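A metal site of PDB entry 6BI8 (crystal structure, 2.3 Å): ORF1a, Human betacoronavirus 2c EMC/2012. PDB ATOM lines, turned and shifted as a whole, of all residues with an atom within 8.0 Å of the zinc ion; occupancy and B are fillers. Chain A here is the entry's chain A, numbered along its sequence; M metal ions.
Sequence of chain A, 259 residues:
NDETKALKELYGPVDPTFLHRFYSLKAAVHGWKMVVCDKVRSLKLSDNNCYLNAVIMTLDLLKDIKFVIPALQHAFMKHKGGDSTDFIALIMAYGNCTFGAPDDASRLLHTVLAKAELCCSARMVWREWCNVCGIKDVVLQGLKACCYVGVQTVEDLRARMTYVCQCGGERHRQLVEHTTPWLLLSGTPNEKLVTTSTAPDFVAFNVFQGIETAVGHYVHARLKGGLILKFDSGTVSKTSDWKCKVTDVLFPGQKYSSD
The zinc ion is bound by SG of Cys 133 (2.2 Å), SG of Cys 167 (2.4 Å), SG of Cys 130 (2.4 Å) and SG of Cys 165 (2.5 Å).
The zinc ion has four donor atoms within binding distance.
Within 4 Å of the zinc ion: Cys 130, Cys 133, Cys 165 and Cys 167.
The side-chain sulfur of Cys 165 lies close to the guanidinium group of Arg 171, at 3.4 Å.
N of Val 132 sits close to SG of Cys 130.
SG of Cys 167 sits close to N of Gly 169 (3.3 Å).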
ATOM      1  N   TRP A 129       0.145 -29.169   7.355  1.00  0.00           N
ATOM      2  CA  TRP A 129       0.456 -28.032   8.201  1.00  0.00           C
ATOM      3  C   TRP A 129      -0.729 -27.529   9.002  1.00  0.00           C
ATOM      4  O   TRP A 129      -1.898 -27.672   8.619  1.00  0.00           O
ATOM      5  CB  TRP A 129       1.056 -26.885   7.377  1.00  0.00           C
ATOM      6  CG  TRP A 129       0.121 -26.183   6.436  1.00  0.00           C
ATOM      7  CD1 TRP A 129      -0.541 -25.006   6.669  1.00  0.00           C
ATOM      8  CD2 TRP A 129      -0.212 -26.571   5.102  1.00  0.00           C
ATOM      9  NE1 TRP A 129      -1.281 -24.652   5.568  1.00  0.00           N
ATOM     10  CE2 TRP A 129      -1.094 -25.597   4.589  1.00  0.00           C
ATOM     11  CE3 TRP A 129       0.154 -27.653   4.290  1.00  0.00           C
ATOM     12  CZ2 TRP A 129      -1.637 -25.674   3.308  1.00  0.00           C
ATOM     13  CZ3 TRP A 129      -0.388 -27.731   3.009  1.00  0.00           C
ATOM     14  CH2 TRP A 129      -1.275 -26.746   2.530  1.00  0.00           C
ATOM     15  N   CYS A 130      -0.367 -26.961  10.155  1.00  0.00           N
ATOM     16  CA  CYS A 130      -1.292 -26.366  11.117  1.00  0.00           C
ATOM     17  C   CYS A 130      -0.743 -25.001  11.507  1.00  0.00           C
ATOM     18  O   CYS A 130       0.473 -24.847  11.699  1.00  0.00           O
ATOM     19  CB  CYS A 130      -1.448 -27.289  12.337  1.00  0.00           C
ATOM     20  SG  CYS A 130      -2.542 -26.675  13.662  1.00  0.00           S
ATOM     21  N   ASN A 131      -1.621 -23.998  11.594  1.00  0.00           N
ATOM     22  CA  ASN A 131      -1.177 -22.646  11.967  1.00  0.00           C
ATOM     23  C   ASN A 131      -0.525 -22.670  13.337  1.00  0.00           C
ATOM     24  O   ASN A 131       0.420 -21.937  13.609  1.00  0.00           O
ATOM     25  CB  ASN A 131      -2.341 -21.653  11.956  1.00  0.00           C
ATOM     26  CG  ASN A 131      -2.841 -21.353  10.570  1.00  0.00           C
ATOM     27  OD1 ASN A 131      -2.139 -21.595   9.580  1.00  0.00           O
ATOM     28  ND2 ASN A 131      -4.066 -20.829  10.474  1.00  0.00           N
ATOM     29  N   VAL A 132      -1.058 -23.527  14.202  1.00  0.00           N
ATOM     30  CA  VAL A 132      -0.521 -23.713  15.536  1.00  0.00           C
ATOM     31  C   VAL A 132       0.625 -24.709  15.533  1.00  0.00           C
ATOM     32  O   VAL A 132       1.730 -24.393  15.963  1.00  0.00           O
ATOM     33  CB  VAL A 132      -1.630 -24.185  16.514  1.00  0.00           C
ATOM     34  CG1 VAL A 132      -1.007 -24.767  17.794  1.00  0.00           C
ATOM     35  CG2 VAL A 132      -2.597 -23.039  16.828  1.00  0.00           C
ATOM     36  N   CYS A 133       0.366 -25.925  15.026  1.00  0.00           N
ATOM     37  CA  CYS A 133       1.300 -27.039  15.198  1.00  0.00           C
ATOM     38  C   CYS A 133       2.518 -27.038  14.252  1.00  0.00           C
ATOM     39  O   CYS A 133       3.518 -27.707  14.535  1.00  0.00           O
ATOM     40  CB  CYS A 133       0.544 -28.363  15.037  1.00  0.00           C
ATOM     41  SG  CYS A 133      -0.680 -28.674  16.348  1.00  0.00           S
ATOM     42  N   GLY A 134       2.453 -26.288  13.166  1.00  0.00           N
ATOM     43  CA  GLY A 134       3.582 -26.212  12.251  1.00  0.00           C
ATOM     44  C   GLY A 134       3.504 -27.146  11.048  1.00  0.00           C
ATOM     45  O   GLY A 134       2.436 -27.660  10.714  1.00  0.00           O
ATOM     46  N   VAL A 164      -9.337 -31.699  10.498  1.00  0.00           N
ATOM     47  CA  VAL A 164      -9.127 -31.155  11.826  1.00  0.00           C
ATOM     48  C   VAL A 164      -7.863 -31.764  12.414  1.00  0.00           C
ATOM     49  O   VAL A 164      -7.626 -32.956  12.334  1.00  0.00           O
ATOM     50  CB  VAL A 164     -10.352 -31.372  12.751  1.00  0.00           C
ATOM     51  CG1 VAL A 164     -11.646 -31.261  11.938  1.00  0.00           C
ATOM     52  CG2 VAL A 164     -10.271 -32.687  13.472  1.00  0.00           C
ATOM     53  N   CYS A 165      -7.040 -30.900  12.974  1.00  0.00           N
ATOM     54  CA  CYS A 165      -5.766 -31.307  13.536  1.00  0.00           C
ATOM     55  C   CYS A 165      -5.984 -31.890  14.928  1.00  0.00           C
ATOM     56  O   CYS A 165      -7.032 -31.700  15.535  1.00  0.00           O
ATOM     57  CB  CYS A 165      -4.803 -30.113  13.593  1.00  0.00           C
ATOM     58  SG  CYS A 165      -3.184 -30.509  14.287  1.00  0.00           S
ATOM     59  N   GLN A 166      -4.974 -32.611  15.409  1.00  0.00           N
ATOM     60  CA  GLN A 166      -4.948 -33.129  16.781  1.00  0.00           C
ATOM     61  C   GLN A 166      -5.310 -32.056  17.797  1.00  0.00           C
ATOM     62  O   GLN A 166      -5.991 -32.328  18.781  1.00  0.00           O
ATOM     63  CB  GLN A 166      -3.562 -33.671  17.114  1.00  0.00           C
ATOM     64  CG  GLN A 166      -3.315 -35.082  16.709  1.00  0.00           C
ATOM     65  CD  GLN A 166      -2.173 -35.681  17.501  1.00  0.00           C
ATOM     66  OE1 GLN A 166      -2.376 -36.544  18.371  1.00  0.00           O
ATOM     67  NE2 GLN A 166      -0.955 -35.226  17.221  1.00  0.00           N
ATOM     68  N   CYS A 167      -4.827 -30.846  17.549  1.00  0.00           N
ATOM     69  CA  CYS A 167      -4.907 -29.757  18.510  1.00  0.00           C
ATOM     70  C   CYS A 167      -6.286 -29.097  18.558  1.00  0.00           C
ATOM     71  O   CYS A 167      -6.525 -28.221  19.393  1.00  0.00           O
ATOM     72  CB  CYS A 167      -3.858 -28.699  18.188  1.00  0.00           C
ATOM     73  SG  CYS A 167      -4.340 -27.694  16.769  1.00  0.00           S
ATOM     74  N   GLY A 168      -7.174 -29.491  17.653  1.00  0.00           N
ATOM     75  CA  GLY A 168      -8.489 -28.885  17.565  1.00  0.00           C
ATOM     76  C   GLY A 168      -8.611 -27.871  16.437  1.00  0.00           C
ATOM     77  O   GLY A 168      -9.720 -27.613  15.943  1.00  0.00           O
ATOM     78  N   GLY A 169      -7.480 -27.305  16.015  1.00  0.00           N
ATOM     79  CA  GLY A 169      -7.476 -26.353  14.924  1.00  0.00           C
ATOM     80  C   GLY A 169      -7.621 -27.027  13.577  1.00  0.00           C
ATOM     81  O   GLY A 169      -7.644 -28.252  13.490  1.00  0.00           O
ATOM     82  N   GLU A 170      -7.737 -26.249  12.502  1.00  0.00           N
ATOM     83  CA  GLU A 170      -7.878 -26.867  11.187  1.00  0.00           C
ATOM     84  C   GLU A 170      -6.492 -27.223  10.638  1.00  0.00           C
ATOM     85  O   GLU A 170      -5.514 -26.501  10.854  1.00  0.00           O
ATOM     86  CB  GLU A 170      -8.641 -25.955  10.228  1.00  0.00           C
ATOM     87  CG  GLU A 170      -7.825 -24.869   9.583  1.00  0.00           C
ATOM     88  CD  GLU A 170      -8.651 -24.003   8.656  1.00  0.00           C
ATOM     89  OE1 GLU A 170      -9.769 -24.433   8.300  1.00  0.00           O
ATOM     90  OE2 GLU A 170      -8.197 -22.898   8.300  1.00  0.00           O
ATOM     91  N   ARG A 171      -6.412 -28.353   9.952  1.00  0.00           N
ATOM     92  CA  ARG A 171      -5.138 -28.813   9.414  1.00  0.00           C
ATOM     93  C   ARG A 171      -5.244 -28.965   7.911  1.00  0.00           C
ATOM     94  O   ARG A 171      -6.332 -29.191   7.369  1.00  0.00           O
ATOM     95  CB  ARG A 171      -4.701 -30.133  10.067  1.00  0.00           C
ATOM     96  CG  ARG A 171      -3.511 -30.789   9.390  1.00  0.00           C
ATOM     97  CD  ARG A 171      -2.841 -31.838  10.278  1.00  0.00           C
ATOM     98  NE  ARG A 171      -1.883 -31.226  11.195  1.00  0.00           N
ATOM     99  CZ  ARG A 171      -0.601 -31.588  11.293  1.00  0.00           C
ATOM    100  NH1 ARG A 171      -0.120 -32.564  10.549  1.00  0.00           N
ATOM    101  NH2 ARG A 171       0.182 -30.959  12.153  1.00  0.00           N
HETATM  102 ZN    ZN M   1      -2.609 -28.346  15.317  1.00  0.00          ZN
